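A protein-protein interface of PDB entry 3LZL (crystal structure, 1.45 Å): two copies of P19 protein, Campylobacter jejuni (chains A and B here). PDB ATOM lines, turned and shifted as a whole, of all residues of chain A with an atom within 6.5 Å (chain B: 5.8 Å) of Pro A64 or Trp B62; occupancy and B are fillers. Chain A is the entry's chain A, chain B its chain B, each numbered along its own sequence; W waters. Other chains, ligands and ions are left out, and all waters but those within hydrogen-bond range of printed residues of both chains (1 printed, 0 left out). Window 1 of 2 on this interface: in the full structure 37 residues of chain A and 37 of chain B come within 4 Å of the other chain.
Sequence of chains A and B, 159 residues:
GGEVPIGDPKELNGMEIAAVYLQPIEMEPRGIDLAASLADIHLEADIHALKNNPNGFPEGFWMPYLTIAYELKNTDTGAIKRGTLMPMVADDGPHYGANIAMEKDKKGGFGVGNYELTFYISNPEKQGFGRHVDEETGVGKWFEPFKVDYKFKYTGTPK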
ATOM      1  N   ILE A  47      -3.126 -25.456  -5.041  1.00  0.00           N
ATOM      2  CA  ILE A  47      -2.093 -24.481  -5.312  1.00  0.00           C
ATOM      3  C   ILE A  47      -1.379 -24.153  -4.000  1.00  0.00           C
ATOM      4  O   ILE A  47      -1.993 -23.610  -3.073  1.00  0.00           O
ATOM      5  CB  ILE A  47      -2.635 -23.157  -5.933  1.00  0.00           C
ATOM      6  CG1 ILE A  47      -3.571 -23.528  -7.092  1.00  0.00           C
ATOM      7  CG2 ILE A  47      -1.466 -22.260  -6.393  1.00  0.00           C
ATOM      8  CD1 ILE A  47      -4.162 -22.339  -7.816  1.00  0.00           C
ATOM      9  N   PHE A  57       5.698 -16.709   0.776  1.00  0.00           N
ATOM     10  CA  PHE A  57       4.833 -17.754   1.352  1.00  0.00           C
ATOM     11  C   PHE A  57       5.632 -18.982   1.764  1.00  0.00           C
ATOM     12  O   PHE A  57       6.438 -19.474   0.969  1.00  0.00           O
ATOM     13  CB  PHE A  57       3.745 -18.173   0.366  1.00  0.00           C
ATOM     14  CG  PHE A  57       2.583 -17.245   0.393  1.00  0.00           C
ATOM     15  CD1 PHE A  57       2.597 -16.083  -0.314  1.00  0.00           C
ATOM     16  CD2 PHE A  57       1.467 -17.559   1.190  1.00  0.00           C
ATOM     17  CE1 PHE A  57       1.515 -15.209  -0.206  1.00  0.00           C
ATOM     18  CE2 PHE A  57       0.384 -16.692   1.252  1.00  0.00           C
ATOM     19  CZ  PHE A  57       0.470 -15.525   0.567  1.00  0.00           C
ATOM     20  N   PHE A  61       2.352 -23.839   2.170  1.00  0.00           N
ATOM     21  CA  PHE A  61       1.181 -23.017   2.459  1.00  0.00           C
ATOM     22  C   PHE A  61       0.292 -22.951   1.218  1.00  0.00           C
ATOM     23  O   PHE A  61       0.783 -22.870   0.074  1.00  0.00           O
ATOM     24  CB  PHE A  61       1.559 -21.582   2.890  1.00  0.00           C
ATOM     25  CG  PHE A  61       1.656 -21.387   4.368  1.00  0.00           C
ATOM     26  CD1 PHE A  61       1.986 -22.441   5.236  1.00  0.00           C
ATOM     27  CD2 PHE A  61       1.457 -20.104   4.917  1.00  0.00           C
ATOM     28  CE1 PHE A  61       2.054 -22.221   6.629  1.00  0.00           C
ATOM     29  CE2 PHE A  61       1.540 -19.892   6.309  1.00  0.00           C
ATOM     30  CZ  PHE A  61       1.850 -20.963   7.149  1.00  0.00           C
ATOM     31  N   TRP A  62      -0.991 -22.880   1.460  1.00  0.00           N
ATOM     32  CA  TRP A  62      -1.982 -22.626   0.463  1.00  0.00           C
ATOM     33  C   TRP A  62      -1.778 -21.195  -0.060  1.00  0.00           C
ATOM     34  O   TRP A  62      -1.451 -20.289   0.714  1.00  0.00           O
ATOM     35  CB  TRP A  62      -3.397 -22.777   1.097  1.00  0.00           C
ATOM     36  CG  TRP A  62      -4.474 -22.588   0.042  1.00  0.00           C
ATOM     37  CD1 TRP A  62      -4.634 -23.274  -1.124  1.00  0.00           C
ATOM     38  CD2 TRP A  62      -5.547 -21.623   0.090  1.00  0.00           C
ATOM     39  NE1 TRP A  62      -5.721 -22.798  -1.814  1.00  0.00           N
ATOM     40  CE2 TRP A  62      -6.308 -21.784  -1.101  1.00  0.00           C
ATOM     41  CE3 TRP A  62      -5.918 -20.632   1.012  1.00  0.00           C
ATOM     42  CZ2 TRP A  62      -7.442 -21.019  -1.383  1.00  0.00           C
ATOM     43  CZ3 TRP A  62      -7.052 -19.869   0.739  1.00  0.00           C
ATOM     44  CH2 TRP A  62      -7.812 -20.070  -0.442  1.00  0.00           C
ATOM     45  N   MET A  63      -1.888 -21.006  -1.362  1.00  0.00           N
ATOM     46  CA  MET A  63      -1.773 -19.691  -1.987  1.00  0.00           C
ATOM     47  C   MET A  63      -3.156 -19.032  -2.052  1.00  0.00           C
ATOM     48  O   MET A  63      -4.005 -19.464  -2.860  1.00  0.00           O
ATOM     49  CB  MET A  63      -1.201 -19.830  -3.380  1.00  0.00           C
ATOM     50  CG  MET A  63       0.186 -20.414  -3.429  1.00  0.00           C
ATOM     51  SD  MET A  63       1.468 -19.516  -2.537  1.00  0.00           S
ATOM     52  CE  MET A  63       1.438 -17.963  -3.415  1.00  0.00           C
ATOM     53  N   PRO A  64      -3.401 -18.020  -1.194  1.00  0.00           N
ATOM     54  CA  PRO A  64      -4.739 -17.446  -1.022  1.00  0.00           C
ATOM     55  C   PRO A  64      -4.939 -16.222  -1.922  1.00  0.00           C
ATOM     56  O   PRO A  64      -3.986 -15.671  -2.499  1.00  0.00           O
ATOM     57  CB  PRO A  64      -4.708 -17.027   0.440  1.00  0.00           C
ATOM     58  CG  PRO A  64      -3.306 -16.507   0.632  1.00  0.00           C
ATOM     59  CD  PRO A  64      -2.435 -17.345  -0.291  1.00  0.00           C
ATOM     60  N   TYR A  65      -6.183 -15.789  -2.040  1.00  0.00           N
ATOM     61  CA  TYR A  65      -6.585 -14.548  -2.730  1.00  0.00           C
ATOM     62  C   TYR A  65      -6.289 -14.548  -4.232  1.00  0.00           C
ATOM     63  O   TYR A  65      -6.300 -13.505  -4.859  1.00  0.00           O
ATOM     64  CB  TYR A  65      -5.978 -13.312  -2.046  1.00  0.00           C
ATOM     65  CG  TYR A  65      -6.449 -13.090  -0.649  1.00  0.00           C
ATOM     66  CD1 TYR A  65      -5.802 -13.632   0.432  1.00  0.00           C
ATOM     67  CD2 TYR A  65      -7.511 -12.290  -0.388  1.00  0.00           C
ATOM     68  CE1 TYR A  65      -6.253 -13.433   1.710  1.00  0.00           C
ATOM     69  CE2 TYR A  65      -7.971 -12.091   0.904  1.00  0.00           C
ATOM     70  CZ  TYR A  65      -7.330 -12.661   1.956  1.00  0.00           C
ATOM     71  OH  TYR A  65      -7.713 -12.457   3.248  1.00  0.00           O
ATOM     72  N   LEU A  66      -6.101 -15.735  -4.834  1.00  0.00           N
ATOM     73  CA  LEU A  66      -5.915 -15.827  -6.266  1.00  0.00           C
ATOM     74  C   LEU A  66      -7.244 -15.702  -6.985  1.00  0.00           C
ATOM     75  O   LEU A  66      -8.285 -16.086  -6.454  1.00  0.00           O
ATOM     76  CB  LEU A  66      -5.289 -17.157  -6.643  1.00  0.00           C
ATOM     77  CG  LEU A  66      -3.920 -17.421  -6.045  1.00  0.00           C
ATOM     78  CD1 LEU A  66      -3.416 -18.798  -6.494  1.00  0.00           C
ATOM     79  CD2 LEU A  66      -2.950 -16.342  -6.572  1.00  0.00           C
ATOM     80  N   PRO A  94      -7.926 -25.885   2.543  1.00  0.00           N
ATOM     81  CA  PRO A  94      -8.426 -24.901   1.569  1.00  0.00           C
ATOM     82  C   PRO A  94      -7.984 -25.254   0.176  1.00  0.00           C
ATOM     83  O   PRO A  94      -6.917 -25.894  -0.017  1.00  0.00           O
ATOM     84  CB  PRO A  94      -7.764 -23.606   2.022  1.00  0.00           C
ATOM     85  CG  PRO A  94      -6.497 -24.045   2.707  1.00  0.00           C
ATOM     86  CD  PRO A  94      -6.897 -25.295   3.428  1.00  0.00           C
ATOM     87  N   TYR A  96      -9.286 -24.117  -4.332  1.00  0.00           N
ATOM     88  CA  TYR A  96     -10.181 -23.410  -5.232  1.00  0.00           C
ATOM     89  C   TYR A  96     -10.969 -24.467  -5.970  1.00  0.00           C
ATOM     90  O   TYR A  96     -10.384 -25.440  -6.471  1.00  0.00           O
ATOM     91  CB  TYR A  96      -9.353 -22.564  -6.231  1.00  0.00           C
ATOM     92  CG  TYR A  96      -8.527 -21.485  -5.582  1.00  0.00           C
ATOM     93  CD1 TYR A  96      -9.021 -20.244  -5.330  1.00  0.00           C
ATOM     94  CD2 TYR A  96      -7.220 -21.724  -5.236  1.00  0.00           C
ATOM     95  CE1 TYR A  96      -8.278 -19.260  -4.694  1.00  0.00           C
ATOM     96  CE2 TYR A  96      -6.456 -20.770  -4.607  1.00  0.00           C
ATOM     97  CZ  TYR A  96      -6.987 -19.503  -4.364  1.00  0.00           C
ATOM     98  OH  TYR A  96      -6.277 -18.527  -3.722  1.00  0.00           O
ATOM     99  N   ASN A 123      -2.823 -12.670  -9.744  1.00  0.00           N
ATOM    100  CA  ASN A 123      -2.226 -12.563  -8.439  1.00  0.00           C
ATOM    101  C   ASN A 123      -3.132 -11.946  -7.357  1.00  0.00           C
ATOM    102  O   ASN A 123      -4.152 -11.344  -7.691  1.00  0.00           O
ATOM    103  CB  ASN A 123      -0.864 -11.862  -8.524  1.00  0.00           C
ATOM    104  CG  ASN A 123      -0.982 -10.351  -8.787  1.00  0.00           C
ATOM    105  OD1 ASN A 123      -1.729  -9.671  -8.106  1.00  0.00           O
ATOM    106  ND2 ASN A 123      -0.178  -9.828  -9.733  1.00  0.00           N
ATOM    107  N   PRO A 124      -2.760 -12.091  -6.076  1.00  0.00           N
ATOM    108  CA  PRO A 124      -3.632 -11.622  -5.025  1.00  0.00           C
ATOM    109  C   PRO A 124      -3.897 -10.106  -4.989  1.00  0.00           C
ATOM    110  O   PRO A 124      -4.827  -9.684  -4.330  1.00  0.00           O
ATOM    111  CB  PRO A 124      -2.869 -12.026  -3.751  1.00  0.00           C
ATOM    112  CG  PRO A 124      -2.103 -13.216  -4.139  1.00  0.00           C
ATOM    113  CD  PRO A 124      -1.624 -12.850  -5.521  1.00  0.00           C
ATOM    114  N   GLN A 127      -7.281  -8.690  -5.677  1.00  0.00           N
ATOM    115  CA  GLN A 127      -8.237  -8.752  -4.576  1.00  0.00           C
ATOM    116  C   GLN A 127      -7.810  -8.001  -3.320  1.00  0.00           C
ATOM    117  O   GLN A 127      -8.274  -8.301  -2.228  1.00  0.00           O
ATOM    118  CB  GLN A 127      -8.534 -10.194  -4.186  1.00  0.00           C
ATOM    119  CG  GLN A 127      -9.127 -10.977  -5.344  1.00  0.00           C
ATOM    120  CD  GLN A 127      -9.530 -12.384  -4.972  1.00  0.00           C
ATOM    121  OE1 GLN A 127      -9.643 -12.719  -3.791  1.00  0.00           O
ATOM    122  NE2 GLN A 127      -9.722 -13.239  -5.991  1.00  0.00           N
ATOM    123  N   PHE A 129      -4.864  -7.729  -1.724  1.00  0.00           N
ATOM    124  CA  PHE A 129      -3.847  -8.323  -0.864  1.00  0.00           C
ATOM    125  C   PHE A 129      -2.571  -7.563  -1.082  1.00  0.00           C
ATOM    126  O   PHE A 129      -2.161  -7.333  -2.213  1.00  0.00           O
ATOM    127  CB  PHE A 129      -3.727  -9.789  -1.268  1.00  0.00           C
ATOM    128  CG  PHE A 129      -2.831 -10.620  -0.371  1.00  0.00           C
ATOM    129  CD1 PHE A 129      -1.501 -10.693  -0.619  1.00  0.00           C
ATOM    130  CD2 PHE A 129      -3.345 -11.270   0.706  1.00  0.00           C
ATOM    131  CE1 PHE A 129      -0.685 -11.469   0.224  1.00  0.00           C
ATOM    132  CE2 PHE A 129      -2.537 -12.003   1.577  1.00  0.00           C
ATOM    133  CZ  PHE A 129      -1.212 -12.098   1.306  1.00  0.00           C
ATOM    134  N   TRP A 142       4.715  -9.744  -7.758  1.00  0.00           N
ATOM    135  CA  TRP A 142       3.876 -10.868  -8.142  1.00  0.00           C
ATOM    136  C   TRP A 142       3.911 -11.131  -9.630  1.00  0.00           C
ATOM    137  O   TRP A 142       4.075 -10.214 -10.414  1.00  0.00           O
ATOM    138  CB  TRP A 142       2.418 -10.643  -7.743  1.00  0.00           C
ATOM    139  CG  TRP A 142       2.095 -10.801  -6.347  1.00  0.00           C
ATOM    140  CD1 TRP A 142       1.858  -9.832  -5.507  1.00  0.00           C
ATOM    141  CD2 TRP A 142       1.979 -12.051  -5.619  1.00  0.00           C
ATOM    142  NE1 TRP A 142       1.537 -10.349  -4.271  1.00  0.00           N
ATOM    143  CE2 TRP A 142       1.656 -11.714  -4.313  1.00  0.00           C
ATOM    144  CE3 TRP A 142       2.120 -13.406  -5.960  1.00  0.00           C
ATOM    145  CZ2 TRP A 142       1.433 -12.645  -3.330  1.00  0.00           C
ATOM    146  CZ3 TRP A 142       1.884 -14.384  -4.956  1.00  0.00           C
ATOM    147  CH2 TRP A 142       1.558 -13.982  -3.662  1.00  0.00           C
ATOM    148  N   ALA B  45      -1.652  -8.724  13.175  1.00  0.00           N
ATOM    149  CA  ALA B  45      -2.318  -9.822  13.817  1.00  0.00           C
ATOM    150  C   ALA B  45      -1.786 -11.090  13.147  1.00  0.00           C
ATOM    151  O   ALA B  45      -1.808 -11.190  11.904  1.00  0.00           O
ATOM    152  CB  ALA B  45      -3.844  -9.757  13.594  1.00  0.00           C
ATOM    153  N   ILE B  47      -2.401 -14.981  12.914  1.00  0.00           N
ATOM    154  CA  ILE B  47      -3.492 -15.897  13.155  1.00  0.00           C
ATOM    155  C   ILE B  47      -3.327 -17.171  12.346  1.00  0.00           C
ATOM    156  O   ILE B  47      -3.321 -17.127  11.115  1.00  0.00           O
ATOM    157  CB  ILE B  47      -4.848 -15.246  12.766  1.00  0.00           C
ATOM    158  CG1 ILE B  47      -4.999 -13.890  13.462  1.00  0.00           C
ATOM    159  CG2 ILE B  47      -5.986 -16.175  13.145  1.00  0.00           C
ATOM    160  CD1 ILE B  47      -6.357 -13.217  13.244  1.00  0.00           C
ATOM    161  N   HIS B  48      -3.137 -18.284  13.052  1.00  0.00           N
ATOM    162  CA  HIS B  48      -2.879 -19.582  12.427  1.00  0.00           C
ATOM    163  C   HIS B  48      -3.729 -20.668  13.054  1.00  0.00           C
ATOM    164  O   HIS B  48      -4.127 -20.551  14.209  1.00  0.00           O
ATOM    165  CB  HIS B  48      -1.389 -19.950  12.521  1.00  0.00           C
ATOM    166  CG  HIS B  48      -0.498 -18.974  11.831  1.00  0.00           C
ATOM    167  ND1 HIS B  48      -0.112 -17.789  12.410  1.00  0.00           N
ATOM    168  CD2 HIS B  48       0.059 -18.998  10.613  1.00  0.00           C
ATOM    169  CE1 HIS B  48       0.629 -17.111  11.547  1.00  0.00           C
ATOM    170  NE2 HIS B  48       0.730 -17.814  10.445  1.00  0.00           N
ATOM    171  N   ALA B  49      -3.981 -21.743  12.283  1.00  0.00           N
ATOM    172  CA  ALA B  49      -4.766 -22.842  12.780  1.00  0.00           C
ATOM    173  C   ALA B  49      -4.017 -23.630  13.861  1.00  0.00           C
ATOM    174  O   ALA B  49      -2.834 -23.902  13.752  1.00  0.00           O
ATOM    175  CB  ALA B  49      -5.146 -23.784  11.651  1.00  0.00           C
ATOM    176  N   PHE B  57      -8.685 -26.566   8.546  1.00  0.00           N
ATOM    177  CA  PHE B  57      -7.381 -25.980   8.324  1.00  0.00           C
ATOM    178  C   PHE B  57      -6.269 -26.780   9.013  1.00  0.00           C
ATOM    179  O   PHE B  57      -6.362 -27.031  10.249  1.00  0.00           O
ATOM    180  CB  PHE B  57      -7.323 -24.507   8.719  1.00  0.00           C
ATOM    181  CG  PHE B  57      -7.905 -23.580   7.686  1.00  0.00           C
ATOM    182  CD1 PHE B  57      -9.248 -23.384   7.574  1.00  0.00           C
ATOM    183  CD2 PHE B  57      -7.091 -22.997   6.737  1.00  0.00           C
ATOM    184  CE1 PHE B  57      -9.740 -22.587   6.553  1.00  0.00           C
ATOM    185  CE2 PHE B  57      -7.597 -22.190   5.755  1.00  0.00           C
ATOM    186  CZ  PHE B  57      -8.896 -22.021   5.661  1.00  0.00           C
ATOM    187  N   GLY B  60      -1.003 -24.911  11.816  1.00  0.00           N
ATOM    188  CA  GLY B  60       0.006 -24.030  11.328  1.00  0.00           C
ATOM    189  C   GLY B  60      -0.335 -23.147  10.162  1.00  0.00           C
ATOM    190  O   GLY B  60       0.347 -22.147   9.870  1.00  0.00           O
ATOM    191  N   PHE B  61      -1.370 -23.538   9.432  1.00  0.00           N
ATOM    192  CA  PHE B  61      -1.765 -22.745   8.266  1.00  0.00           C
ATOM    193  C   PHE B  61      -2.235 -21.377   8.692  1.00  0.00           C
ATOM    194  O   PHE B  61      -2.945 -21.242   9.665  1.00  0.00           O
ATOM    195  CB  PHE B  61      -2.880 -23.413   7.435  1.00  0.00           C
ATOM    196  CG  PHE B  61      -2.418 -24.235   6.260  1.00  0.00           C
ATOM    197  CD1 PHE B  61      -1.159 -24.818   6.192  1.00  0.00           C
ATOM    198  CD2 PHE B  61      -3.285 -24.406   5.180  1.00  0.00           C
ATOM    199  CE1 PHE B  61      -0.784 -25.601   5.097  1.00  0.00           C
ATOM    200  CE2 PHE B  61      -2.913 -25.135   4.080  1.00  0.00           C
ATOM    201  CZ  PHE B  61      -1.663 -25.728   4.022  1.00  0.00           C
ATOM    202  N   TRP B  62      -1.914 -20.376   7.882  1.00  0.00           N
ATOM    203  CA  TRP B  62      -2.491 -19.068   8.067  1.00  0.00           C
ATOM    204  C   TRP B  62      -3.996 -19.119   7.837  1.00  0.00           C
ATOM    205  O   TRP B  62      -4.466 -19.830   6.926  1.00  0.00           O
ATOM    206  CB  TRP B  62      -1.871 -18.109   7.064  1.00  0.00           C
ATOM    207  CG  TRP B  62      -2.338 -16.717   7.204  1.00  0.00           C
ATOM    208  CD1 TRP B  62      -2.206 -15.938   8.269  1.00  0.00           C
ATOM    209  CD2 TRP B  62      -2.915 -15.903   6.169  1.00  0.00           C
ATOM    210  NE1 TRP B  62      -2.726 -14.688   8.031  1.00  0.00           N
ATOM    211  CE2 TRP B  62      -3.164 -14.629   6.742  1.00  0.00           C
ATOM    212  CE3 TRP B  62      -3.236 -16.118   4.824  1.00  0.00           C
ATOM    213  CZ2 TRP B  62      -3.699 -13.574   6.010  1.00  0.00           C
ATOM    214  CZ3 TRP B  62      -3.806 -15.078   4.099  1.00  0.00           C
ATOM    215  CH2 TRP B  62      -4.039 -13.829   4.693  1.00  0.00           C
ATOM    216  N   MET B  63      -4.760 -18.407   8.673  1.00  0.00           N
ATOM    217  CA  MET B  63      -6.204 -18.297   8.511  1.00  0.00           C
ATOM    218  C   MET B  63      -6.563 -17.137   7.588  1.00  0.00           C
ATOM    219  O   MET B  63      -6.403 -15.988   8.007  1.00  0.00           O
ATOM    220  CB  MET B  63      -6.898 -18.126   9.828  1.00  0.00           C
ATOM    221  CG  MET B  63      -6.616 -19.236  10.832  1.00  0.00           C
ATOM    222  SD  MET B  63      -7.178 -20.852  10.319  1.00  0.00           S
ATOM    223  CE  MET B  63      -8.917 -20.546  10.100  1.00  0.00           C
ATOM    224  N   PRO B  64      -6.997 -17.424   6.351  1.00  0.00           N
ATOM    225  CA  PRO B  64      -7.221 -16.383   5.342  1.00  0.00           C
ATOM    226  C   PRO B  64      -8.663 -15.876   5.323  1.00  0.00           C
ATOM    227  O   PRO B  64      -9.563 -16.540   5.859  1.00  0.00           O
ATOM    228  CB  PRO B  64      -6.886 -17.132   4.058  1.00  0.00           C
ATOM    229  CG  PRO B  64      -7.514 -18.490   4.283  1.00  0.00           C
ATOM    230  CD  PRO B  64      -7.258 -18.780   5.774  1.00  0.00           C
ATOM    231  N   TYR B  65      -8.861 -14.749   4.648  1.00  0.00           N
ATOM    232  CA  TYR B  65     -10.174 -14.157   4.431  1.00  0.00           C
ATOM    233  C   TYR B  65     -10.905 -13.752   5.701  1.00  0.00           C
ATOM    234  O   TYR B  65     -12.129 -13.575   5.687  1.00  0.00           O
ATOM    235  CB  TYR B  65     -11.059 -15.077   3.580  1.00  0.00           C
ATOM    236  CG  TYR B  65     -10.506 -15.379   2.208  1.00  0.00           C
ATOM    237  CD1 TYR B  65     -10.819 -14.611   1.118  1.00  0.00           C
ATOM    238  CD2 TYR B  65      -9.758 -16.518   1.987  1.00  0.00           C
ATOM    239  CE1 TYR B  65     -10.328 -14.921  -0.138  1.00  0.00           C
ATOM    240  CE2 TYR B  65      -9.265 -16.824   0.750  1.00  0.00           C
ATOM    241  CZ  TYR B  65      -9.540 -16.040  -0.308  1.00  0.00           C
ATOM    242  OH  TYR B  65      -9.056 -16.442  -1.521  1.00  0.00           O
ATOM    243  N   PRO B  87      -5.042  -7.995   4.741  1.00  0.00           N
ATOM    244  CA  PRO B  87      -4.177  -9.149   4.458  1.00  0.00           C
ATOM    245  C   PRO B  87      -3.008  -8.785   3.555  1.00  0.00           C
ATOM    246  O   PRO B  87      -3.142  -7.964   2.628  1.00  0.00           O
ATOM    247  CB  PRO B  87      -5.090 -10.095   3.702  1.00  0.00           C
ATOM    248  CG  PRO B  87      -6.020  -9.206   2.997  1.00  0.00           C
ATOM    249  CD  PRO B  87      -6.271  -8.061   3.956  1.00  0.00           C
ATOM    250  N   MET B  88      -1.852  -9.315   3.886  1.00  0.00           N
ATOM    251  CA  MET B  88      -0.647  -9.018   3.139  1.00  0.00           C
ATOM    252  C   MET B  88       0.408 -10.059   3.448  1.00  0.00           C
ATOM    253  O   MET B  88       0.246 -10.919   4.309  1.00  0.00           O
ATOM    254  CB  MET B  88      -0.118  -7.615   3.528  1.00  0.00           C
ATOM    255  CG  MET B  88       0.297  -7.534   4.970  1.00  0.00           C
ATOM    256  SD  MET B  88       0.856  -5.874   5.423  1.00  0.00           S
ATOM    257  CE  MET B  88      -0.779  -5.051   5.614  1.00  0.00           C
ATOM    258  N   PRO B  94       2.339 -14.657   5.236  1.00  0.00           N
ATOM    259  CA  PRO B  94       1.172 -13.787   5.309  1.00  0.00           C
ATOM    260  C   PRO B  94       0.744 -13.401   6.753  1.00  0.00           C
ATOM    261  O   PRO B  94       0.963 -14.152   7.689  1.00  0.00           O
ATOM    262  CB  PRO B  94       0.089 -14.609   4.608  1.00  0.00           C
ATOM    263  CG  PRO B  94       0.495 -16.071   4.922  1.00  0.00           C
ATOM    264  CD  PRO B  94       1.989 -16.043   4.853  1.00  0.00           C
ATOM    265  N   HIS B  95       0.130 -12.240   6.875  1.00  0.00           N
ATOM    266  CA  HIS B  95      -0.474 -11.763   8.103  1.00  0.00           C
ATOM    267  C   HIS B  95      -1.500 -10.697   7.788  1.00  0.00           C
ATOM    268  O   HIS B  95      -1.764 -10.397   6.610  1.00  0.00           O
ATOM    269  CB  HIS B  95       0.599 -11.208   9.039  1.00  0.00           C
ATOM    270  CG  HIS B  95       1.349 -10.054   8.465  1.00  0.00           C
ATOM    271  ND1 HIS B  95       2.557 -10.203   7.808  1.00  0.00           N
ATOM    272  CD2 HIS B  95       1.047  -8.741   8.408  1.00  0.00           C
ATOM    273  CE1 HIS B  95       2.976  -9.015   7.411  1.00  0.00           C
ATOM    274  NE2 HIS B  95       2.072  -8.121   7.744  1.00  0.00           N
ATOM    275  N   TYR B  96      -2.111 -10.140   8.840  1.00  0.00           N
ATOM    276  CA  TYR B  96      -3.033  -8.995   8.704  1.00  0.00           C
ATOM    277  C   TYR B  96      -2.369  -7.805   9.357  1.00  0.00           C
ATOM    278  O   TYR B  96      -1.774  -7.960  10.400  1.00  0.00           O
ATOM    279  CB  TYR B  96      -4.372  -9.275   9.376  1.00  0.00           C
ATOM    280  CG  TYR B  96      -5.115 -10.443   8.811  1.00  0.00           C
ATOM    281  CD1 TYR B  96      -5.994 -10.287   7.761  1.00  0.00           C
ATOM    282  CD2 TYR B  96      -4.967 -11.722   9.341  1.00  0.00           C
ATOM    283  CE1 TYR B  96      -6.657 -11.349   7.224  1.00  0.00           C
ATOM    284  CE2 TYR B  96      -5.664 -12.812   8.815  1.00  0.00           C
ATOM    285  CZ  TYR B  96      -6.511 -12.617   7.740  1.00  0.00           C
ATOM    286  OH  TYR B  96      -7.212 -13.657   7.163  1.00  0.00           O
HETATM  287  O   HOH W   1      -9.941 -15.379  -3.598  1.00  0.00           O
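OH of Tyr A65 sits at hydrogen-bond distance from N of Tyr B65 (2.9 Å).
The backbone NH of Tyr A65 is in hydrogen-bond range of the side-chain hydroxyl of Tyr A96, 3.2 Å away.
The backbone carbonyl oxygen (O) of Pro A124 sits close to the backbone NH (N) of Phe A129 (3.3 Å).
The backbone carbonyl oxygen of Ala B49 sits at hydrogen-bond distance from the backbone NH of Gly B60 (2.8 Å).
The backbone NH (N) of Ala B49 lies within hydrogen-bond range of the backbone carbonyl oxygen (O) of Phe B61.
The side-chain hydroxyl (OH) of Tyr B96 sits at hydrogen-bond distance from the backbone NH (N) of Tyr B65, 3.2 Å away.
CE2 of Phe A57 touches CG of Pro B94, 3.7 Å away.
Phe B61 touches Trp A62.
Trp A62 touches Pro B64 (CZ3 to CG, 3.8 Å).
Pro A64 touches Trp B62.
Tyr A65 touches Pro B87.
CG of Pro A94 touches CE2 of Phe B57, at 3.7 Å.
Phe B61 touches Pro A94.
Trp B62 touches Phe A129 (CH2 to CE2, 3.9 Å).
O of Pro B87 touches CA of Phe A129, 3.6 Å away.
Phe A129 touches Met B88 (CZ to C, 3.4 Å).
Of the printed residues of chain B, Trp A62 touches Phe B61, Pro B64 and Tyr B65.
Of chain B, only Trp B62 (3.8 Å) comes within 4 Å of Pro A64.
Of the printed residues of chain A, Phe B57 touches Pro A94 (3.7 Å).
Of the printed residues of chain A, Phe B61 touches Trp A62 and Pro A94.
Of chain A, only Phe A61, Pro A64, Tyr A65 and Phe A129 come within 4 Å of Trp B62.
Of the printed residues of chain A, Tyr B65 touches Trp A62 (3.8 Å) and Tyr A65 (2.9 Å).
Printed residues of chain A within 4 Å of Met B88: Phe A129.
The nearest residue of chain B that does not touch Pro A64 is Tyr B65 (4.1 Å).
The nearest printed residue of chain A that does not touch Pro B87 is Gln A127 (5.8 Å).
Of the 15 printed residues of chain A, 7 touch a printed residue of chain B.
Hydrophobic or aromatic side chains of chain A within 4 Å of the printed part of chain B: Phe A57, Phe A61, Trp A62, Pro A64, Tyr A65, Pro A94 and Phe A129.
Printed residues of chain B that touch a printed residue of chain A: Phe B57, Gly B60, Phe B61, Trp B62, Pro B64, Tyr B65, Pro B87, Met B88 and Pro B94.
Hydrophobic or aromatic side chains of chain B within 4 Å of the printed part of chain A: Phe B57, Phe B61, Trp B62, Pro B64, Tyr B65, Pro B87 and Pro B94.
Among the printed residues, 15 pairs touch across the chains.
Among the printed residues, no Asp or Glu carboxylate lies within 4 Å of a Lys or Arg side-chain nitrogen of the other chain.
Phe A57 touches Pro B94, and with the chains exchanged Pro A94 touches Phe B57.
Trp A62 touches Pro B64, and with the chains exchanged Pro A64 touches Trp B62.
Trp A62 touches Tyr B65, and with the chains exchanged Tyr A65 touches Trp B62.
Tyr B65 touches its own counterpart, Tyr A65.
9 positions are printed for both chains.
Of the 15 pairs that touch across the chains among the printed residues, 9 have their exchanged pair printed and touching as well.
Water W1 lies within hydrogen-bond range of the side-chain hydroxyl (OH) of Tyr B65 (2.5 Å), the side-chain amide oxygen (OE1) of Gln A127 (2.7 Å) and the backbone carbonyl oxygen (O) of Leu A66 (3.4 Å).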
